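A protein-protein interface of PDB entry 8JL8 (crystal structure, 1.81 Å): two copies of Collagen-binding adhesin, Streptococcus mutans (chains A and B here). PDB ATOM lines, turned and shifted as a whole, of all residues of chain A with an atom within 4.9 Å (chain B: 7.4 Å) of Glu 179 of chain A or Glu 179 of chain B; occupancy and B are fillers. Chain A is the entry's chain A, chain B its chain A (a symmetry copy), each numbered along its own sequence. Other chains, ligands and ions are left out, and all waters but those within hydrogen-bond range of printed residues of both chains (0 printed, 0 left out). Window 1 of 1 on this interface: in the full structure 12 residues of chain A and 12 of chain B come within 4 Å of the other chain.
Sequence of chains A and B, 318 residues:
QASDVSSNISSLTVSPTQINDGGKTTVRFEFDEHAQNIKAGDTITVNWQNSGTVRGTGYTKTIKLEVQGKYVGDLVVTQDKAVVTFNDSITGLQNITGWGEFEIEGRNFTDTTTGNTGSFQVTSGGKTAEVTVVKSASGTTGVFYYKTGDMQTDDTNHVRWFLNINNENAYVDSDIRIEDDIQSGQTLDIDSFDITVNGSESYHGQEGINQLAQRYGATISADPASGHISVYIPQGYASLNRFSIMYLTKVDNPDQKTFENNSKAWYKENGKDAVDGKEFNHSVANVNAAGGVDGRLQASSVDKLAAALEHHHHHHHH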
ATOM      1  N   ARG A 177      -1.653   5.009  21.646  1.00  0.00           N
ATOM      2  CA  ARG A 177      -0.501   4.096  21.807  1.00  0.00           C
ATOM      3  C   ARG A 177       0.690   4.922  22.258  1.00  0.00           C
ATOM      4  O   ARG A 177       0.966   5.996  21.663  1.00  0.00           O
ATOM      5  CB  ARG A 177      -0.217   3.343  20.503  1.00  0.00           C
ATOM      6  CG  ARG A 177      -1.461   2.682  19.942  1.00  0.00           C
ATOM      7  CD  ARG A 177      -1.202   1.803  18.747  1.00  0.00           C
ATOM      8  NE  ARG A 177      -0.375   2.410  17.708  1.00  0.00           N
ATOM      9  CZ  ARG A 177      -0.808   3.140  16.690  1.00  0.00           C
ATOM     10  NH1 ARG A 177      -2.087   3.412  16.543  1.00  0.00           N
ATOM     11  NH2 ARG A 177       0.060   3.606  15.814  1.00  0.00           N
ATOM     12  N   ILE A 178       1.318   4.468  23.339  1.00  0.00           N
ATOM     13  CA  ILE A 178       2.616   5.020  23.786  1.00  0.00           C
ATOM     14  C   ILE A 178       3.642   3.877  23.731  1.00  0.00           C
ATOM     15  O   ILE A 178       3.335   2.795  24.208  1.00  0.00           O
ATOM     16  CB  ILE A 178       2.548   5.640  25.195  1.00  0.00           C
ATOM     17  CG1 ILE A 178       1.245   6.393  25.504  1.00  0.00           C
ATOM     18  CG2 ILE A 178       3.799   6.479  25.418  1.00  0.00           C
ATOM     19  CD1 ILE A 178       1.026   7.702  24.820  1.00  0.00           C
ATOM     20  N   GLU A 179       4.830   4.176  23.228  1.00  0.00           N
ATOM     21  CA  GLU A 179       6.021   3.297  23.183  1.00  0.00           C
ATOM     22  C   GLU A 179       7.134   4.058  23.913  1.00  0.00           C
ATOM     23  O   GLU A 179       7.489   5.183  23.513  1.00  0.00           O
ATOM     24  CB  GLU A 179       6.325   2.915  21.720  1.00  0.00           C
ATOM     25  CG  GLU A 179       5.236   2.044  21.083  1.00  0.00           C
ATOM     26  CD  GLU A 179       4.965   0.700  21.711  1.00  0.00           C
ATOM     27  OE1 GLU A 179       5.733   0.295  22.590  1.00  0.00           O
ATOM     28  OE2 GLU A 179       3.972   0.023  21.302  1.00  0.00           O
ATOM     29  N   ASP A 180       7.610   3.502  25.016  1.00  0.00           N
ATOM     30  CA  ASP A 180       8.508   4.225  25.942  1.00  0.00           C
ATOM     31  C   ASP A 180       9.809   3.429  26.076  1.00  0.00           C
ATOM     32  O   ASP A 180       9.732   2.245  26.308  1.00  0.00           O
ATOM     33  CB  ASP A 180       7.756   4.467  27.257  1.00  0.00           C
ATOM     34  CG  ASP A 180       8.530   5.310  28.241  1.00  0.00           C
ATOM     35  OD1 ASP A 180       9.649   4.917  28.578  1.00  0.00           O
ATOM     36  OD2 ASP A 180       8.001   6.360  28.637  1.00  0.00           O
ATOM     37  N   ASP A 181      10.947   4.065  25.818  1.00  0.00           N
ATOM     38  CA  ASP A 181      12.272   3.493  26.120  1.00  0.00           C
ATOM     39  C   ASP A 181      12.924   4.310  27.245  1.00  0.00           C
ATOM     40  O   ASP A 181      13.350   5.472  27.024  1.00  0.00           O
ATOM     41  CB  ASP A 181      13.120   3.386  24.851  1.00  0.00           C
ATOM     42  CG  ASP A 181      12.530   2.374  23.880  1.00  0.00           C
ATOM     43  OD1 ASP A 181      12.733   1.143  24.083  1.00  0.00           O
ATOM     44  OD2 ASP A 181      11.801   2.812  23.024  1.00  0.00           O
ATOM     45  N   HIS A 228      11.712  -1.106  28.187  1.00  0.00           N
ATOM     46  CA  HIS A 228      10.591  -0.756  27.296  1.00  0.00           C
ATOM     47  C   HIS A 228       9.269  -0.870  28.055  1.00  0.00           C
ATOM     48  O   HIS A 228       9.069  -1.816  28.845  1.00  0.00           O
ATOM     49  CB  HIS A 228      10.615  -1.578  25.998  1.00  0.00           C
ATOM     50  CG  HIS A 228       9.745  -0.933  24.989  1.00  0.00           C
ATOM     51  ND1 HIS A 228      10.201   0.057  24.153  1.00  0.00           N
ATOM     52  CD2 HIS A 228       8.420  -1.042  24.773  1.00  0.00           C
ATOM     53  CE1 HIS A 228       9.188   0.487  23.413  1.00  0.00           C
ATOM     54  NE2 HIS A 228       8.082  -0.157  23.788  1.00  0.00           N
ATOM     55  N   ILE A 229       8.403   0.105  27.818  1.00  0.00           N
ATOM     56  CA  ILE A 229       6.987   0.088  28.252  1.00  0.00           C
ATOM     57  C   ILE A 229       6.100   0.395  27.045  1.00  0.00           C
ATOM     58  O   ILE A 229       6.397   1.320  26.327  1.00  0.00           O
ATOM     59  CB  ILE A 229       6.690   1.100  29.365  1.00  0.00           C
ATOM     60  CG1 ILE A 229       7.653   0.967  30.545  1.00  0.00           C
ATOM     61  CG2 ILE A 229       5.205   0.948  29.759  1.00  0.00           C
ATOM     62  CD1 ILE A 229       7.635   2.163  31.491  1.00  0.00           C
ATOM     63  N   SER A 230       5.037  -0.378  26.871  1.00  0.00           N
ATOM     64  CA  SER A 230       4.033  -0.174  25.813  1.00  0.00           C
ATOM     65  C   SER A 230       2.715   0.144  26.511  1.00  0.00           C
ATOM     66  O   SER A 230       2.392  -0.518  27.508  1.00  0.00           O
ATOM     67  CB  SER A 230       3.934  -1.397  24.937  1.00  0.00           C
ATOM     68  OG  SER A 230       5.224  -1.732  24.427  1.00  0.00           O
ATOM     69  N   ASN A 262      12.419   8.323  27.101  1.00  0.00           N
ATOM     70  CA  ASN A 262      11.958   8.667  25.732  1.00  0.00           C
ATOM     71  C   ASN A 262      10.603   8.007  25.500  1.00  0.00           C
ATOM     72  O   ASN A 262      10.461   6.844  25.830  1.00  0.00           O
ATOM     73  CB  ASN A 262      12.992   8.240  24.693  1.00  0.00           C
ATOM     74  CG  ASN A 262      14.294   8.999  24.811  1.00  0.00           C
ATOM     75  OD1 ASN A 262      14.399   9.952  25.565  1.00  0.00           O
ATOM     76  ND2 ASN A 262      15.300   8.582  24.065  1.00  0.00           N
ATOM     77  N   SER A 263       9.663   8.711  24.879  1.00  0.00           N
ATOM     78  CA  SER A 263       8.416   8.082  24.413  1.00  0.00           C
ATOM     79  C   SER A 263       8.094   8.588  23.010  1.00  0.00           C
ATOM     80  O   SER A 263       8.659   9.629  22.574  1.00  0.00           O
ATOM     81  CB  SER A 263       7.259   8.249  25.349  1.00  0.00           C
ATOM     82  OG  SER A 263       6.853   9.586  25.424  1.00  0.00           O
ATOM     83  N   LYS A 264       7.268   7.806  22.343  1.00  0.00           N
ATOM     84  CA  LYS A 264       6.570   8.190  21.096  1.00  0.00           C
ATOM     85  C   LYS A 264       5.088   7.906  21.313  1.00  0.00           C
ATOM     86  O   LYS A 264       4.730   6.921  21.979  1.00  0.00           O
ATOM     87  CB  LYS A 264       7.172   7.448  19.898  1.00  0.00           C
ATOM     88  CG  LYS A 264       8.590   7.860  19.542  1.00  0.00           C
ATOM     89  CD  LYS A 264       9.154   7.108  18.343  1.00  0.00           C
ATOM     90  CE  LYS A 264      10.580   7.493  18.027  1.00  0.00           C
ATOM     91  NZ  LYS A 264      10.761   7.717  16.575  1.00  0.00           N
ATOM     92  N   TRP A 266       0.967   7.867  19.510  1.00  0.00           N
ATOM     93  CA  TRP A 266       0.012   7.809  18.379  1.00  0.00           C
ATOM     94  C   TRP A 266      -1.377   7.996  18.962  1.00  0.00           C
ATOM     95  O   TRP A 266      -1.736   7.225  19.864  1.00  0.00           O
ATOM     96  CB  TRP A 266       0.077   6.483  17.615  1.00  0.00           C
ATOM     97  CG  TRP A 266       1.364   6.197  16.903  1.00  0.00           C
ATOM     98  CD1 TRP A 266       1.603   6.269  15.564  1.00  0.00           C
ATOM     99  CD2 TRP A 266       2.570   5.691  17.494  1.00  0.00           C
ATOM    100  NE1 TRP A 266       2.899   5.906  15.285  1.00  0.00           N
ATOM    101  CE2 TRP A 266       3.510   5.530  16.451  1.00  0.00           C
ATOM    102  CE3 TRP A 266       2.966   5.431  18.808  1.00  0.00           C
ATOM    103  CZ2 TRP A 266       4.803   5.059  16.685  1.00  0.00           C
ATOM    104  CZ3 TRP A 266       4.254   5.009  19.040  1.00  0.00           C
ATOM    105  CH2 TRP A 266       5.149   4.797  17.995  1.00  0.00           C
ATOM    106  N   TYR B 145      -0.675 -16.270  14.031  1.00  0.00           N
ATOM    107  CA  TYR B 145       0.618 -15.566  14.242  1.00  0.00           C
ATOM    108  C   TYR B 145       1.632 -16.510  14.870  1.00  0.00           C
ATOM    109  O   TYR B 145       1.306 -17.190  15.847  1.00  0.00           O
ATOM    110  CB  TYR B 145       0.432 -14.327  15.119  1.00  0.00           C
ATOM    111  CG  TYR B 145       1.744 -13.715  15.560  1.00  0.00           C
ATOM    112  CD1 TYR B 145       2.609 -13.129  14.644  1.00  0.00           C
ATOM    113  CD2 TYR B 145       2.173 -13.818  16.879  1.00  0.00           C
ATOM    114  CE1 TYR B 145       3.814 -12.568  15.045  1.00  0.00           C
ATOM    115  CE2 TYR B 145       3.374 -13.268  17.288  1.00  0.00           C
ATOM    116  CZ  TYR B 145       4.216 -12.678  16.364  1.00  0.00           C
ATOM    117  OH  TYR B 145       5.400 -12.169  16.789  1.00  0.00           O
ATOM    118  N   LYS B 147       6.306 -16.387  15.306  1.00  0.00           N
ATOM    119  CA  LYS B 147       7.622 -15.794  15.024  1.00  0.00           C
ATOM    120  C   LYS B 147       8.582 -16.958  14.807  1.00  0.00           C
ATOM    121  O   LYS B 147       8.534 -17.976  15.564  1.00  0.00           O
ATOM    122  CB  LYS B 147       7.992 -14.832  16.158  1.00  0.00           C
ATOM    123  CG  LYS B 147       9.462 -14.775  16.475  1.00  0.00           C
ATOM    124  CD  LYS B 147       9.849 -13.668  17.430  1.00  0.00           C
ATOM    125  CE  LYS B 147      11.023 -12.923  16.855  1.00  0.00           C
ATOM    126  NZ  LYS B 147      11.475 -11.801  17.689  1.00  0.00           N
ATOM    127  N   LEU B 163       8.174 -12.202  11.560  1.00  0.00           N
ATOM    128  CA  LEU B 163       6.908 -12.042  12.317  1.00  0.00           C
ATOM    129  C   LEU B 163       5.809 -12.305  11.306  1.00  0.00           C
ATOM    130  O   LEU B 163       5.581 -11.433  10.440  1.00  0.00           O
ATOM    131  CB  LEU B 163       6.810 -10.660  12.974  1.00  0.00           C
ATOM    132  CG  LEU B 163       8.069 -10.150  13.669  1.00  0.00           C
ATOM    133  CD1 LEU B 163       7.847  -8.755  14.231  1.00  0.00           C
ATOM    134  CD2 LEU B 163       8.524 -11.087  14.774  1.00  0.00           C
ATOM    135  N   ARG B 177      -1.531  -5.962  17.497  1.00  0.00           N
ATOM    136  CA  ARG B 177      -0.361  -5.327  18.142  1.00  0.00           C
ATOM    137  C   ARG B 177       0.648  -6.418  18.454  1.00  0.00           C
ATOM    138  O   ARG B 177       0.268  -7.478  19.012  1.00  0.00           O
ATOM    139  CB  ARG B 177      -0.782  -4.558  19.398  1.00  0.00           C
ATOM    140  CG  ARG B 177      -1.934  -3.609  19.128  1.00  0.00           C
ATOM    141  CD  ARG B 177      -2.281  -2.720  20.294  1.00  0.00           C
ATOM    142  NE  ARG B 177      -2.413  -3.410  21.573  1.00  0.00           N
ATOM    143  CZ  ARG B 177      -3.520  -3.955  22.057  1.00  0.00           C
ATOM    144  NH1 ARG B 177      -4.644  -3.939  21.370  1.00  0.00           N
ATOM    145  NH2 ARG B 177      -3.492  -4.529  23.243  1.00  0.00           N
ATOM    146  N   ILE B 178       1.884  -6.187  18.019  1.00  0.00           N
ATOM    147  CA  ILE B 178       3.030  -7.032  18.420  1.00  0.00           C
ATOM    148  C   ILE B 178       4.021  -6.131  19.174  1.00  0.00           C
ATOM    149  O   ILE B 178       4.307  -5.047  18.690  1.00  0.00           O
ATOM    150  CB  ILE B 178       3.709  -7.725  17.222  1.00  0.00           C
ATOM    151  CG1 ILE B 178       2.744  -8.207  16.127  1.00  0.00           C
ATOM    152  CG2 ILE B 178       4.621  -8.824  17.750  1.00  0.00           C
ATOM    153  CD1 ILE B 178       1.882  -9.386  16.436  1.00  0.00           C
ATOM    154  N   GLU B 179       4.556  -6.637  20.275  1.00  0.00           N
ATOM    155  CA  GLU B 179       5.623  -6.029  21.103  1.00  0.00           C
ATOM    156  C   GLU B 179       6.757  -7.060  21.152  1.00  0.00           C
ATOM    157  O   GLU B 179       6.545  -8.202  21.601  1.00  0.00           O
ATOM    158  CB  GLU B 179       5.041  -5.614  22.470  1.00  0.00           C
ATOM    159  CG  GLU B 179       4.006  -4.488  22.370  1.00  0.00           C
ATOM    160  CD  GLU B 179       4.467  -3.167  21.808  1.00  0.00           C
ATOM    161  OE1 GLU B 179       5.676  -2.999  21.614  1.00  0.00           O
ATOM    162  OE2 GLU B 179       3.604  -2.267  21.572  1.00  0.00           O
ATOM    163  N   ASP B 180       7.912  -6.699  20.614  1.00  0.00           N
ATOM    164  CA  ASP B 180       9.010  -7.663  20.380  1.00  0.00           C
ATOM    165  C   ASP B 180      10.252  -7.172  21.128  1.00  0.00           C
ATOM    166  O   ASP B 180      10.586  -6.018  20.986  1.00  0.00           O
ATOM    167  CB  ASP B 180       9.189  -7.836  18.867  1.00  0.00           C
ATOM    168  CG  ASP B 180      10.202  -8.893  18.503  1.00  0.00           C
ATOM    169  OD1 ASP B 180      11.345  -8.772  18.949  1.00  0.00           O
ATOM    170  OD2 ASP B 180       9.819  -9.834  17.790  1.00  0.00           O
ATOM    171  N   ASP B 181      10.828  -8.013  21.981  1.00  0.00           N
ATOM    172  CA  ASP B 181      12.144  -7.758  22.594  1.00  0.00           C
ATOM    173  C   ASP B 181      13.156  -8.775  22.046  1.00  0.00           C
ATOM    174  O   ASP B 181      13.101  -9.982  22.396  1.00  0.00           O
ATOM    175  CB  ASP B 181      12.038  -7.741  24.121  1.00  0.00           C
ATOM    176  CG  ASP B 181      11.209  -6.558  24.599  1.00  0.00           C
ATOM    177  OD1 ASP B 181      11.748  -5.416  24.654  1.00  0.00           O
ATOM    178  OD2 ASP B 181      10.037  -6.767  24.796  1.00  0.00           O
ATOM    179  N   SER B 221       7.770   0.474  14.550  1.00  0.00           N
ATOM    180  CA  SER B 221       8.677   1.372  15.286  1.00  0.00           C
ATOM    181  C   SER B 221       9.741   0.500  15.967  1.00  0.00           C
ATOM    182  O   SER B 221       9.375  -0.537  16.548  1.00  0.00           O
ATOM    183  CB  SER B 221       7.829   2.172  16.236  1.00  0.00           C
ATOM    184  OG  SER B 221       8.589   3.217  16.810  1.00  0.00           O
ATOM    185  N   HIS B 228      13.953  -3.309  20.960  1.00  0.00           N
ATOM    186  CA  HIS B 228      12.480  -3.347  20.952  1.00  0.00           C
ATOM    187  C   HIS B 228      11.960  -3.012  19.554  1.00  0.00           C
ATOM    188  O   HIS B 228      12.491  -2.107  18.879  1.00  0.00           O
ATOM    189  CB  HIS B 228      11.878  -2.457  22.050  1.00  0.00           C
ATOM    190  CG  HIS B 228      10.462  -2.827  22.265  1.00  0.00           C
ATOM    191  ND1 HIS B 228      10.090  -3.827  23.130  1.00  0.00           N
ATOM    192  CD2 HIS B 228       9.342  -2.425  21.634  1.00  0.00           C
ATOM    193  CE1 HIS B 228       8.774  -3.977  23.064  1.00  0.00           C
ATOM    194  NE2 HIS B 228       8.296  -3.143  22.139  1.00  0.00           N
ATOM    195  N   ILE B 229      10.948  -3.763  19.140  1.00  0.00           N
ATOM    196  CA  ILE B 229      10.137  -3.478  17.934  1.00  0.00           C
ATOM    197  C   ILE B 229       8.658  -3.501  18.320  1.00  0.00           C
ATOM    198  O   ILE B 229       8.250  -4.412  18.999  1.00  0.00           O
ATOM    199  CB  ILE B 229      10.377  -4.483  16.801  1.00  0.00           C
ATOM    200  CG1 ILE B 229      11.860  -4.643  16.469  1.00  0.00           C
ATOM    201  CG2 ILE B 229       9.517  -4.050  15.594  1.00  0.00           C
ATOM    202  CD1 ILE B 229      12.172  -5.875  15.625  1.00  0.00           C
ATOM    203  N   SER B 230       7.904  -2.510  17.864  1.00  0.00           N
ATOM    204  CA  SER B 230       6.449  -2.419  18.070  1.00  0.00           C
ATOM    205  C   SER B 230       5.802  -2.501  16.691  1.00  0.00           C
ATOM    206  O   SER B 230       6.306  -1.861  15.756  1.00  0.00           O
ATOM    207  CB  SER B 230       6.097  -1.142  18.789  1.00  0.00           C
ATOM    208  OG  SER B 230       6.840  -1.050  20.004  1.00  0.00           O
ATOM    209  N   VAL B 231       4.724  -3.261  16.596  1.00  0.00           N
ATOM    210  CA  VAL B 231       3.928  -3.404  15.347  1.00  0.00           C
ATOM    211  C   VAL B 231       2.474  -3.120  15.726  1.00  0.00           C
ATOM    212  O   VAL B 231       2.002  -3.689  16.726  1.00  0.00           O
ATOM    213  CB  VAL B 231       4.100  -4.788  14.691  1.00  0.00           C
ATOM    214  CG1 VAL B 231       3.192  -4.941  13.479  1.00  0.00           C
ATOM    215  CG2 VAL B 231       5.546  -5.034  14.278  1.00  0.00           C
ATOM    216  N   TYR B 232       1.882  -2.188  14.993  1.00  0.00           N
ATOM    217  CA  TYR B 232       0.461  -1.816  15.016  1.00  0.00           C
ATOM    218  C   TYR B 232      -0.106  -1.921  13.589  1.00  0.00           C
ATOM    219  O   TYR B 232       0.380  -1.212  12.677  1.00  0.00           O
ATOM    220  CB  TYR B 232       0.307  -0.397  15.562  1.00  0.00           C
ATOM    221  CG  TYR B 232      -1.147  -0.057  15.722  1.00  0.00           C
ATOM    222  CD1 TYR B 232      -1.874  -0.624  16.750  1.00  0.00           C
ATOM    223  CD2 TYR B 232      -1.819   0.709  14.776  1.00  0.00           C
ATOM    224  CE1 TYR B 232      -3.231  -0.377  16.886  1.00  0.00           C
ATOM    225  CE2 TYR B 232      -3.172   0.975  14.906  1.00  0.00           C
ATOM    226  CZ  TYR B 232      -3.883   0.415  15.957  1.00  0.00           C
ATOM    227  OH  TYR B 232      -5.223   0.632  16.124  1.00  0.00           O
ATOM    228  N   ASN B 262      11.834 -12.569  21.557  1.00  0.00           N
ATOM    229  CA  ASN B 262      10.573 -12.706  22.328  1.00  0.00           C
ATOM    230  C   ASN B 262       9.537 -11.759  21.732  1.00  0.00           C
ATOM    231  O   ASN B 262       9.876 -10.620  21.470  1.00  0.00           O
ATOM    232  CB  ASN B 262      10.817 -12.433  23.811  1.00  0.00           C
ATOM    233  CG  ASN B 262      11.721 -13.456  24.458  1.00  0.00           C
ATOM    234  OD1 ASN B 262      12.060 -14.462  23.858  1.00  0.00           O
ATOM    235  ND2 ASN B 262      12.120 -13.208  25.692  1.00  0.00           N
ATOM    236  N   SER B 263       8.292 -12.201  21.595  1.00  0.00           N
ATOM    237  CA  SER B 263       7.189 -11.289  21.246  1.00  0.00           C
ATOM    238  C   SER B 263       5.978 -11.612  22.118  1.00  0.00           C
ATOM    239  O   SER B 263       5.923 -12.713  22.730  1.00  0.00           O
ATOM    240  CB  SER B 263       6.844 -11.276  19.789  1.00  0.00           C
ATOM    241  OG  SER B 263       6.297 -12.499  19.383  1.00  0.00           O
ATOM    242  N   LYS B 264       5.107 -10.626  22.196  1.00  0.00           N
ATOM    243  CA  LYS B 264       3.731 -10.761  22.723  1.00  0.00           C
ATOM    244  C   LYS B 264       2.793 -10.186  21.668  1.00  0.00           C
ATOM    245  O   LYS B 264       3.135  -9.200  20.997  1.00  0.00           O
ATOM    246  CB  LYS B 264       3.615 -10.077  24.090  1.00  0.00           C
ATOM    247  CG  LYS B 264       4.392 -10.753  25.207  1.00  0.00           C
ATOM    248  CD  LYS B 264       4.248 -10.051  26.552  1.00  0.00           C
ATOM    249  CE  LYS B 264       5.061 -10.705  27.645  1.00  0.00           C
ATOM    250  NZ  LYS B 264       4.263 -10.855  28.883  1.00  0.00           N
ATOM    251  N   ALA B 265       1.614 -10.772  21.540  1.00  0.00           N
ATOM    252  CA  ALA B 265       0.636 -10.390  20.507  1.00  0.00           C
ATOM    253  C   ALA B 265      -0.728 -10.109  21.142  1.00  0.00           C
ATOM    254  O   ALA B 265      -1.080 -10.840  22.057  1.00  0.00           O
ATOM    255  CB  ALA B 265       0.521 -11.488  19.492  1.00  0.00           C
ATOM    256  N   TRP B 266      -1.443  -9.145  20.573  1.00  0.00           N
ATOM    257  CA  TRP B 266      -2.851  -8.803  20.885  1.00  0.00           C
ATOM    258  C   TRP B 266      -3.593  -8.734  19.562  1.00  0.00           C
ATOM    259  O   TRP B 266      -3.152  -7.973  18.688  1.00  0.00           O
ATOM    260  CB  TRP B 266      -2.987  -7.469  21.624  1.00  0.00           C
ATOM    261  CG  TRP B 266      -2.381  -7.410  22.992  1.00  0.00           C
ATOM    262  CD1 TRP B 266      -3.032  -7.432  24.188  1.00  0.00           C
ATOM    263  CD2 TRP B 266      -0.993  -7.215  23.301  1.00  0.00           C
ATOM    264  NE1 TRP B 266      -2.138  -7.332  25.227  1.00  0.00           N
ATOM    265  CE2 TRP B 266      -0.880  -7.180  24.709  1.00  0.00           C
ATOM    266  CE3 TRP B 266       0.168  -7.142  22.526  1.00  0.00           C
ATOM    267  CZ2 TRP B 266       0.350  -7.012  25.349  1.00  0.00           C
ATOM    268  CZ3 TRP B 266       1.381  -7.020  23.161  1.00  0.00           C
ATOM    269  CH2 TRP B 266       1.470  -6.926  24.548  1.00  0.00           C
ATOM    270  N   LYS B 278      -0.304 -12.914  24.603  1.00  0.00           N
ATOM    271  CA  LYS B 278       0.279 -14.273  24.621  1.00  0.00           C
ATOM    272  C   LYS B 278       1.703 -14.160  24.074  1.00  0.00           C
ATOM    273  O   LYS B 278       1.917 -13.309  23.175  1.00  0.00           O
ATOM    274  CB  LYS B 278      -0.545 -15.255  23.796  1.00  0.00           C
ATOM    275  CG  LYS B 278       0.064 -16.640  23.652  1.00  0.00           C
ATOM    276  CD  LYS B 278      -0.937 -17.745  23.842  1.00  0.00           C
ATOM    277  CE  LYS B 278      -0.310 -19.113  23.799  1.00  0.00           C
ATOM    278  NZ  LYS B 278      -0.361 -19.610  22.412  1.00  0.00           N
ATOM    279  N   PHE B 280       5.056 -15.358  22.020  1.00  0.00           N
ATOM    280  CA  PHE B 280       5.441 -16.102  20.798  1.00  0.00           C
ATOM    281  C   PHE B 280       6.935 -15.833  20.649  1.00  0.00           C
ATOM    282  O   PHE B 280       7.277 -14.747  20.189  1.00  0.00           O
ATOM    283  CB  PHE B 280       4.625 -15.635  19.597  1.00  0.00           C
ATOM    284  CG  PHE B 280       3.142 -15.892  19.704  1.00  0.00           C
ATOM    285  CD1 PHE B 280       2.305 -14.969  20.322  1.00  0.00           C
ATOM    286  CD2 PHE B 280       2.589 -17.049  19.185  1.00  0.00           C
ATOM    287  CE1 PHE B 280       0.940 -15.202  20.427  1.00  0.00           C
ATOM    288  CE2 PHE B 280       1.224 -17.272  19.288  1.00  0.00           C
ATOM    289  CZ  PHE B 280       0.409 -16.361  19.929  1.00  0.00           C
ATOM    290  N   ASN B 281       7.744 -16.719  21.218  1.00  0.00           N
ATOM    291  CA  ASN B 281       9.219 -16.593  21.309  1.00  0.00           C
ATOM    292  C   ASN B 281       9.859 -17.576  20.334  1.00  0.00           C
ATOM    293  O   ASN B 281       9.202 -18.579  19.972  1.00  0.00           O
ATOM    294  CB  ASN B 281       9.737 -16.888  22.705  1.00  0.00           C
ATOM    295  CG  ASN B 281       9.076 -16.025  23.753  1.00  0.00           C
ATOM    296  OD1 ASN B 281       8.558 -14.954  23.425  1.00  0.00           O
ATOM    297  ND2 ASN B 281       9.145 -16.467  25.008  1.00  0.00           N
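OE1 of Glu 179 of chain A is in hydrogen-bond range of NE2 of His 228 of chain A, 2.7 Å away. The side-chain carboxylate (OE1) of Glu 179 of chain B lies within hydrogen-bond range of a ring nitrogen (NE2) of His 228 of chain B (2.7 Å). OE1 of Glu 179 of chain B sits at hydrogen-bond distance from OG of Ser 230 of chain B, at 2.8 Å. O of Asp 180 of chain B lies within hydrogen-bond range of ND1 of His 228 of chain B, at 3.1 Å. N of Ser 230 of chain B sits at hydrogen-bond distance from O of Ser 221 of chain B, at 2.8 Å. The side-chain hydroxyl (OG) of Ser 230 of chain B lies close to a ring nitrogen (NE2) of His 228 of chain B (3.3 Å).
Printed residues of chain B within 4 Å of Arg 177 of chain A: Tyr 232 (3.1 Å). Glu 179 of chain A touches just these residues of chain B: Glu 179 and Ser 230. Printed residues of chain B within 4 Å of Trp 266 of chain A: Ser 221. Printed residues of chain A within 4 Å of His 228 of chain B: His 228 (3.4 Å). The nearest residue of chain B that does not touch Glu 179 of chain A is His 228 of chain B (4.3 Å).
OG of Ser 230 of chain B lies close to OE1 of Glu 179 of chain A. A ring nitrogen (NE2) of His 228 of chain B lies close to a ring nitrogen (NE2) of His 228 of chain A, at 3.4 Å. The side-chain hydroxyl of Ser 230 of chain A lies close to the side-chain carboxylate of Glu 179 of chain B (3.1 Å). The side-chain carboxylate of Glu 179 of chain A lies close to the side-chain carboxylate of Glu 179 of chain B (2.3 Å).
Among the printed residues, pairs that only touch across the chains: Arg 177 of chain A with Tyr 232 of chain B (3.1 Å) and Trp 266 of chain A with Ser 221 of chain B (3.97 Å).
Of the 12 printed residues of chain A, 5 touch a printed residue of chain B. Hydrophobic or aromatic side chains of chain A that line the printed part of chain B: His 228 and Trp 266. Of the 22 printed residues of chain B, 5 touch a printed residue of chain A. Hydrophobic or aromatic side chains of chain B within 4 Å of the printed part of chain A: His 228 and Tyr 232. Among the printed residues, 6 pairs touch across the chains. Among the printed residues, no Asp or Glu carboxylate lies within 4 Å of a Lys or Arg side-chain nitrogen of the other chain.
Glu 179 of chain A touches its own counterpart, Glu 179 of chain B. Glu 179 of chain A touches Ser 230 of chain B, and with the chains exchanged Ser 230 of chain A touches Glu 179 of chain B. His 228 of chain B touches its own counterpart, His 228 of chain A. Positions printed for both chains: 177, 178, 179, 180, 181, 228, 229, 230, 262, 263, 264 and 266.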
